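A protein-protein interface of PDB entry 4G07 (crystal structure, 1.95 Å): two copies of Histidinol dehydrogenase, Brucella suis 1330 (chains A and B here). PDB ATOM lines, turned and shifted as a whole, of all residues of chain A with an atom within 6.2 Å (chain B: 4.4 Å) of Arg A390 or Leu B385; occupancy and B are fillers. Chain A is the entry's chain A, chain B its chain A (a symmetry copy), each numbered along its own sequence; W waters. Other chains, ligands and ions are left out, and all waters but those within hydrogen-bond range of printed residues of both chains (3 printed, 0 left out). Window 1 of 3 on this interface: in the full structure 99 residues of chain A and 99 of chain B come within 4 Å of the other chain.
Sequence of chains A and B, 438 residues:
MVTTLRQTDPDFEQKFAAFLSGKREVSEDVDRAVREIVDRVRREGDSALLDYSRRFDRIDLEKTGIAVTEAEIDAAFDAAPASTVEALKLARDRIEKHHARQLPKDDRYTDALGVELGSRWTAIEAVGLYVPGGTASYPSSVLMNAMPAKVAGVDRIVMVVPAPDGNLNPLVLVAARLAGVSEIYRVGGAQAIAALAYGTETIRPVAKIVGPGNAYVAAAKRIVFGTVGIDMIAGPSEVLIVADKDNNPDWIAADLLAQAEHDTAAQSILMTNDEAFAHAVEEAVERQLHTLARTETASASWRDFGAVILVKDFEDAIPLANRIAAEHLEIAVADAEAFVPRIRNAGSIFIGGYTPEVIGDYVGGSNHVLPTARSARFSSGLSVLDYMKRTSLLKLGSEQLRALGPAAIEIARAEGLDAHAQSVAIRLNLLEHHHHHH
Among the printed residues, merely in contact across the chains: Lys A389 with Ser B380, Thr A391 with Gly B347, Arg A390 with Gln B102, Ser A119 with Gln B102 and Arg A390 with Leu B385.
Printed residues of chain B within 4 Å of Ser A119: Gln B102.
Of the printed residues of chain B, Arg A390 touches Gln B102, Ser B380, Ser B383 and Leu B385.
Of the printed residues of chain B, Thr A391 touches Gly B347.
Printed residues of chain A within 4 Å of Gly B347: Thr A391 (3.5 Å) and Ser A392 (3.1 Å).
Of the printed residues of chain A, Ser B380 touches Lys A389 (3.4 Å) and Arg A390 (2.7 Å).
Of the printed residues of chain A, Ser B383 touches Arg A390.
The nearest residue of chain B that does not touch Arg A390 is Gly B347 (4.1 Å).
The backbone NH (N) of Thr A391 lies within hydrogen-bond range of the backbone carbonyl oxygen (O) of Arg A120, at 2.8 Å.
The side-chain amino group of Lys A389 is in hydrogen-bond range of the side-chain hydroxyl of Thr A122, 2.8 Å away.
The side-chain carboxylate (OD2) of Asp B386 sits at hydrogen-bond distance from the backbone NH (N) of Ser B383.
The guanidinium group (NH1) of Arg A390 is in hydrogen-bond range of the side-chain hydroxyl (OG) of Ser A119 (2.5 Å).
N of Leu B385 sits close to OG of Ser B383 (3.1 Å).
Water W2 lies within hydrogen-bond range of O of Gln B102 (2.7 Å) and NH2 of Arg A390 (3.1 Å).
Water W3 bridges the backbone carbonyl oxygen of Arg A390 and the backbone carbonyl oxygen of Gly B347.
Water W1 lies within hydrogen-bond range of OG of Ser A392 (2.8 Å), O of Gly A118 (3.1 Å) and NE2 of Gln B102 (3.2 Å).
3 positions are printed for both chains.
Of the 8 pairs that touch across the chains among the printed residues, none has its exchanged pair printed and touching as well.
N of Arg A390 sits at hydrogen-bond distance from OG of Ser B380, 2.7 Å away.
NH2 of Arg A390 is in hydrogen-bond range of OG of Ser B383 (3.3 Å).
The backbone NH of Ser A392 is in hydrogen-bond range of the backbone carbonyl oxygen of Gly B347.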
ATOM      1  N   GLY A 118      14.846  20.717   5.983  1.00  0.00           N
ATOM      2  CA  GLY A 118      15.875  20.563   4.977  1.00  0.00           C
ATOM      3  C   GLY A 118      15.477  20.976   3.579  1.00  0.00           C
ATOM      4  O   GLY A 118      14.297  21.028   3.220  1.00  0.00           O
ATOM      5  N   SER A 119      16.503  21.286   2.804  1.00  0.00           N
ATOM      6  CA  SER A 119      16.358  21.690   1.419  1.00  0.00           C
ATOM      7  C   SER A 119      17.503  20.976   0.722  1.00  0.00           C
ATOM      8  O   SER A 119      18.673  21.208   1.048  1.00  0.00           O
ATOM      9  CB  SER A 119      16.531  23.198   1.305  1.00  0.00           C
ATOM     10  OG  SER A 119      16.041  23.648   0.069  1.00  0.00           O
ATOM     11  N   ARG A 120      17.168  20.098  -0.219  1.00  0.00           N
ATOM     12  CA  ARG A 120      18.165  19.336  -0.948  1.00  0.00           C
ATOM     13  C   ARG A 120      17.959  19.428  -2.457  1.00  0.00           C
ATOM     14  O   ARG A 120      16.844  19.270  -2.939  1.00  0.00           O
ATOM     15  CB  ARG A 120      18.097  17.864  -0.554  1.00  0.00           C
ATOM     16  CG  ARG A 120      18.879  17.006  -1.504  1.00  0.00           C
ATOM     17  CD  ARG A 120      18.382  15.619  -1.488  1.00  0.00           C
ATOM     18  NE  ARG A 120      17.213  15.351  -2.329  1.00  0.00           N
ATOM     19  CZ  ARG A 120      16.466  14.268  -2.148  1.00  0.00           C
ATOM     20  NH1 ARG A 120      16.792  13.436  -1.165  1.00  0.00           N
ATOM     21  NH2 ARG A 120      15.435  13.994  -2.938  1.00  0.00           N
ATOM     22  N   TRP A 121      19.041  19.639  -3.199  1.00  0.00           N
ATOM     23  CA  TRP A 121      18.946  19.750  -4.654  1.00  0.00           C
ATOM     24  C   TRP A 121      19.508  18.556  -5.422  1.00  0.00           C
ATOM     25  O   TRP A 121      20.555  18.011  -5.070  1.00  0.00           O
ATOM     26  CB  TRP A 121      19.660  21.016  -5.127  1.00  0.00           C
ATOM     27  CG  TRP A 121      19.001  22.298  -4.657  1.00  0.00           C
ATOM     28  CD1 TRP A 121      19.190  22.940  -3.459  1.00  0.00           C
ATOM     29  CD2 TRP A 121      18.076  23.098  -5.397  1.00  0.00           C
ATOM     30  NE1 TRP A 121      18.440  24.098  -3.417  1.00  0.00           N
ATOM     31  CE2 TRP A 121      17.748  24.216  -4.594  1.00  0.00           C
ATOM     32  CE3 TRP A 121      17.498  22.982  -6.663  1.00  0.00           C
ATOM     33  CZ2 TRP A 121      16.867  25.207  -5.021  1.00  0.00           C
ATOM     34  CZ3 TRP A 121      16.621  23.970  -7.087  1.00  0.00           C
ATOM     35  CH2 TRP A 121      16.317  25.068  -6.270  1.00  0.00           C
ATOM     36  N   THR A 122      18.795  18.134  -6.462  1.00  0.00           N
ATOM     37  CA  THR A 122      19.256  17.042  -7.314  1.00  0.00           C
ATOM     38  C   THR A 122      19.063  17.451  -8.771  1.00  0.00           C
ATOM     39  O   THR A 122      18.255  18.331  -9.089  1.00  0.00           O
ATOM     40  CB  THR A 122      18.474  15.716  -7.076  1.00  0.00           C
ATOM     41  OG1 THR A 122      17.067  15.950  -7.229  1.00  0.00           O
ATOM     42  CG2 THR A 122      18.780  15.141  -5.670  1.00  0.00           C
ATOM     43  N   LEU A 385      19.683  26.017 -12.291  1.00  0.00           N
ATOM     44  CA  LEU A 385      18.471  25.751 -11.511  1.00  0.00           C
ATOM     45  C   LEU A 385      17.355  25.163 -12.358  1.00  0.00           C
ATOM     46  O   LEU A 385      16.498  24.439 -11.850  1.00  0.00           O
ATOM     47  CB  LEU A 385      17.955  27.036 -10.855  1.00  0.00           C
ATOM     48  CG  LEU A 385      18.917  27.722  -9.895  1.00  0.00           C
ATOM     49  CD1 LEU A 385      18.194  28.898  -9.271  1.00  0.00           C
ATOM     50  CD2 LEU A 385      19.379  26.747  -8.829  1.00  0.00           C
ATOM     51  N   MET A 388      17.566  21.323 -12.385  1.00  0.00           N
ATOM     52  CA  MET A 388      17.618  20.701 -11.070  1.00  0.00           C
ATOM     53  C   MET A 388      16.290  20.916 -10.341  1.00  0.00           C
ATOM     54  O   MET A 388      15.442  21.678 -10.806  1.00  0.00           O
ATOM     55  CB  MET A 388      18.758  21.351 -10.267  1.00  0.00           C
ATOM     56  CG  MET A 388      20.141  21.219 -10.929  1.00  0.00           C
ATOM     57  SD  MET A 388      21.464  21.973  -9.899  1.00  0.00           S
ATOM     58  CE  MET A 388      21.801  20.646  -8.748  1.00  0.00           C
ATOM     59  N   LYS A 389      16.086  20.222  -9.218  1.00  0.00           N
ATOM     60  CA  LYS A 389      14.866  20.444  -8.463  1.00  0.00           C
ATOM     61  C   LYS A 389      15.184  20.273  -6.993  1.00  0.00           C
ATOM     62  O   LYS A 389      16.139  19.594  -6.622  1.00  0.00           O
ATOM     63  CB  LYS A 389      13.701  19.521  -8.899  1.00  0.00           C
ATOM     64  CG  LYS A 389      13.846  18.030  -8.570  1.00  0.00           C
ATOM     65  CD  LYS A 389      14.806  17.324  -9.521  1.00  0.00           C
ATOM     66  CE  LYS A 389      14.517  15.819  -9.599  1.00  0.00           C
ATOM     67  NZ  LYS A 389      14.598  15.129  -8.255  1.00  0.00           N
ATOM     68  N   ARG A 390      14.381  20.930  -6.171  1.00  0.00           N
ATOM     69  CA  ARG A 390      14.551  20.914  -4.738  1.00  0.00           C
ATOM     70  C   ARG A 390      13.542  19.969  -4.086  1.00  0.00           C
ATOM     71  O   ARG A 390      12.372  19.896  -4.481  1.00  0.00           O
ATOM     72  CB  ARG A 390      14.354  22.346  -4.189  1.00  0.00           C
ATOM     73  CG  ARG A 390      14.691  22.526  -2.715  1.00  0.00           C
ATOM     74  CD  ARG A 390      13.648  23.423  -2.029  1.00  0.00           C
ATOM     75  NE  ARG A 390      13.557  24.754  -2.621  1.00  0.00           N
ATOM     76  CZ  ARG A 390      14.428  25.736  -2.374  1.00  0.00           C
ATOM     77  NH1 ARG A 390      15.444  25.524  -1.550  1.00  0.00           N
ATOM     78  NH2 ARG A 390      14.290  26.932  -2.942  1.00  0.00           N
ATOM     79  N   THR A 391      14.013  19.233  -3.097  1.00  0.00           N
ATOM     80  CA  THR A 391      13.147  18.345  -2.341  1.00  0.00           C
ATOM     81  C   THR A 391      13.162  18.897  -0.906  1.00  0.00           C
ATOM     82  O   THR A 391      14.228  19.242  -0.393  1.00  0.00           O
ATOM     83  CB  THR A 391      13.681  16.902  -2.355  1.00  0.00           C
ATOM     84  OG1 THR A 391      13.465  16.323  -3.658  1.00  0.00           O
ATOM     85  CG2 THR A 391      12.962  16.054  -1.281  1.00  0.00           C
ATOM     86  N   SER A 392      11.990  19.003  -0.285  1.00  0.00           N
ATOM     87  CA  SER A 392      11.887  19.494   1.092  1.00  0.00           C
ATOM     88  C   SER A 392      12.008  18.305   2.046  1.00  0.00           C
ATOM     89  O   SER A 392      11.474  17.223   1.767  1.00  0.00           O
ATOM     90  CB  SER A 392      10.532  20.174   1.332  1.00  0.00           C
ATOM     91  OG  SER A 392      10.490  21.452   0.742  1.00  0.00           O
ATOM     92  N   GLN B 102      15.306  30.772   2.587  1.00  0.00           N
ATOM     93  CA  GLN B 102      15.575  30.417   1.206  1.00  0.00           C
ATOM     94  C   GLN B 102      15.775  31.604   0.252  1.00  0.00           C
ATOM     95  O   GLN B 102      15.990  31.395  -0.942  1.00  0.00           O
ATOM     96  CB  GLN B 102      14.465  29.468   0.713  1.00  0.00           C
ATOM     97  CG  GLN B 102      14.276  28.257   1.660  1.00  0.00           C
ATOM     98  CD  GLN B 102      13.415  27.116   1.090  1.00  0.00           C
ATOM     99  OE1 GLN B 102      12.578  27.327   0.212  1.00  0.00           O
ATOM    100  NE2 GLN B 102      13.618  25.899   1.611  1.00  0.00           N
ATOM    101  N   PRO B 104      17.306  34.131  -2.143  1.00  0.00           N
ATOM    102  CA  PRO B 104      18.577  34.025  -2.884  1.00  0.00           C
ATOM    103  C   PRO B 104      19.513  35.201  -2.639  1.00  0.00           C
ATOM    104  O   PRO B 104      19.063  36.297  -2.355  1.00  0.00           O
ATOM    105  CB  PRO B 104      18.127  33.963  -4.337  1.00  0.00           C
ATOM    106  CG  PRO B 104      16.911  34.906  -4.342  1.00  0.00           C
ATOM    107  CD  PRO B 104      16.200  34.575  -3.016  1.00  0.00           C
ATOM    108  N   TRP B 121      18.969  39.184  -7.927  1.00  0.00           N
ATOM    109  CA  TRP B 121      17.579  38.749  -7.784  1.00  0.00           C
ATOM    110  C   TRP B 121      16.605  39.854  -7.381  1.00  0.00           C
ATOM    111  O   TRP B 121      16.913  40.693  -6.534  1.00  0.00           O
ATOM    112  CB  TRP B 121      17.490  37.619  -6.760  1.00  0.00           C
ATOM    113  CG  TRP B 121      18.188  36.346  -7.194  1.00  0.00           C
ATOM    114  CD1 TRP B 121      19.516  36.034  -7.050  1.00  0.00           C
ATOM    115  CD2 TRP B 121      17.576  35.212  -7.814  1.00  0.00           C
ATOM    116  NE1 TRP B 121      19.763  34.767  -7.537  1.00  0.00           N
ATOM    117  CE2 TRP B 121      18.589  34.242  -8.012  1.00  0.00           C
ATOM    118  CE3 TRP B 121      16.271  34.917  -8.213  1.00  0.00           C
ATOM    119  CZ2 TRP B 121      18.329  33.003  -8.593  1.00  0.00           C
ATOM    120  CZ3 TRP B 121      16.015  33.682  -8.792  1.00  0.00           C
ATOM    121  CH2 TRP B 121      17.038  32.741  -8.973  1.00  0.00           C
ATOM    122  N   GLY B 347       8.772  15.330  -3.926  1.00  0.00           N
ATOM    123  CA  GLY B 347       8.503  16.742  -3.682  1.00  0.00           C
ATOM    124  C   GLY B 347       8.921  17.103  -2.261  1.00  0.00           C
ATOM    125  O   GLY B 347       9.651  18.073  -2.031  1.00  0.00           O
ATOM    126  N   SER B 380       9.962  21.496  -8.399  1.00  0.00           N
ATOM    127  CA  SER B 380      10.015  21.572  -6.952  1.00  0.00           C
ATOM    128  C   SER B 380       8.721  22.159  -6.451  1.00  0.00           C
ATOM    129  O   SER B 380       7.934  22.696  -7.225  1.00  0.00           O
ATOM    130  CB  SER B 380      11.145  22.486  -6.516  1.00  0.00           C
ATOM    131  OG  SER B 380      12.289  22.286  -7.310  1.00  0.00           O
ATOM    132  N   SER B 383       8.451  27.880  -3.708  1.00  0.00           N
ATOM    133  CA  SER B 383       9.444  28.463  -2.802  1.00  0.00           C
ATOM    134  C   SER B 383       9.552  29.945  -3.167  1.00  0.00           C
ATOM    135  O   SER B 383       8.917  30.383  -4.142  1.00  0.00           O
ATOM    136  CB  SER B 383      10.826  27.799  -2.951  1.00  0.00           C
ATOM    137  OG  SER B 383      11.520  28.299  -4.081  1.00  0.00           O
ATOM    138  N   VAL B 384      10.341  30.713  -2.413  1.00  0.00           N
ATOM    139  CA  VAL B 384      10.463  32.139  -2.728  1.00  0.00           C
ATOM    140  C   VAL B 384      11.012  32.354  -4.140  1.00  0.00           C
ATOM    141  O   VAL B 384      10.755  33.383  -4.766  1.00  0.00           O
ATOM    142  CB  VAL B 384      11.366  32.903  -1.715  1.00  0.00           C
ATOM    143  CG1 VAL B 384      10.695  32.942  -0.347  1.00  0.00           C
ATOM    144  CG2 VAL B 384      12.749  32.258  -1.625  1.00  0.00           C
ATOM    145  N   LEU B 385      11.755  31.375  -4.648  1.00  0.00           N
ATOM    146  CA  LEU B 385      12.333  31.503  -5.989  1.00  0.00           C
ATOM    147  C   LEU B 385      11.271  31.617  -7.068  1.00  0.00           C
ATOM    148  O   LEU B 385      11.510  32.206  -8.123  1.00  0.00           O
ATOM    149  CB  LEU B 385      13.226  30.300  -6.312  1.00  0.00           C
ATOM    150  CG  LEU B 385      14.406  30.081  -5.376  1.00  0.00           C
ATOM    151  CD1 LEU B 385      15.222  28.924  -5.918  1.00  0.00           C
ATOM    152  CD2 LEU B 385      15.248  31.339  -5.289  1.00  0.00           C
ATOM    153  N   ASP B 386      10.102  31.043  -6.811  1.00  0.00           N
ATOM    154  CA  ASP B 386       9.027  31.082  -7.780  1.00  0.00           C
ATOM    155  C   ASP B 386       8.388  32.454  -7.895  1.00  0.00           C
ATOM    156  O   ASP B 386       7.664  32.715  -8.852  1.00  0.00           O
ATOM    157  CB  ASP B 386       7.978  30.026  -7.447  1.00  0.00           C
ATOM    158  CG  ASP B 386       8.536  28.629  -7.557  1.00  0.00           C
ATOM    159  OD1 ASP B 386       9.051  28.299  -8.644  1.00  0.00           O
ATOM    160  OD2 ASP B 386       8.484  27.869  -6.572  1.00  0.00           O
ATOM    161  N   TYR B 387       8.705  33.330  -6.954  1.00  0.00           N
ATOM    162  CA  TYR B 387       8.144  34.677  -6.922  1.00  0.00           C
ATOM    163  C   TYR B 387       9.197  35.751  -7.194  1.00  0.00           C
ATOM    164  O   TYR B 387       8.962  36.949  -6.994  1.00  0.00           O
ATOM    165  CB  TYR B 387       7.512  34.913  -5.556  1.00  0.00           C
ATOM    166  CG  TYR B 387       6.301  34.041  -5.308  1.00  0.00           C
ATOM    167  CD1 TYR B 387       5.125  34.225  -6.032  1.00  0.00           C
ATOM    168  CD2 TYR B 387       6.335  33.021  -4.354  1.00  0.00           C
ATOM    169  CE1 TYR B 387       4.002  33.406  -5.806  1.00  0.00           C
ATOM    170  CE2 TYR B 387       5.225  32.207  -4.126  1.00  0.00           C
ATOM    171  CZ  TYR B 387       4.067  32.405  -4.856  1.00  0.00           C
ATOM    172  OH  TYR B 387       2.982  31.570  -4.647  1.00  0.00           O
ATOM    173  N   MET B 388      10.350  35.302  -7.669  1.00  0.00           N
ATOM    174  CA  MET B 388      11.479  36.181  -7.940  1.00  0.00           C
ATOM    175  C   MET B 388      12.112  35.814  -9.284  1.00  0.00           C
ATOM    176  O   MET B 388      11.764  34.793  -9.876  1.00  0.00           O
ATOM    177  CB  MET B 388      12.516  36.005  -6.817  1.00  0.00           C
ATOM    178  CG  MET B 388      11.972  36.320  -5.412  1.00  0.00           C
ATOM    179  SD  MET B 388      13.271  36.136  -4.123  1.00  0.00           S
ATOM    180  CE  MET B 388      14.099  37.717  -4.244  1.00  0.00           C
HETATM  181  O   HOH W   1      12.174  23.104   2.325  1.00  0.00           O
HETATM  182  O   HOH W   2      16.406  29.102  -2.295  1.00  0.00           O
HETATM  183  O   HOH W   3      10.012  20.628  -3.287  1.00  0.00           O
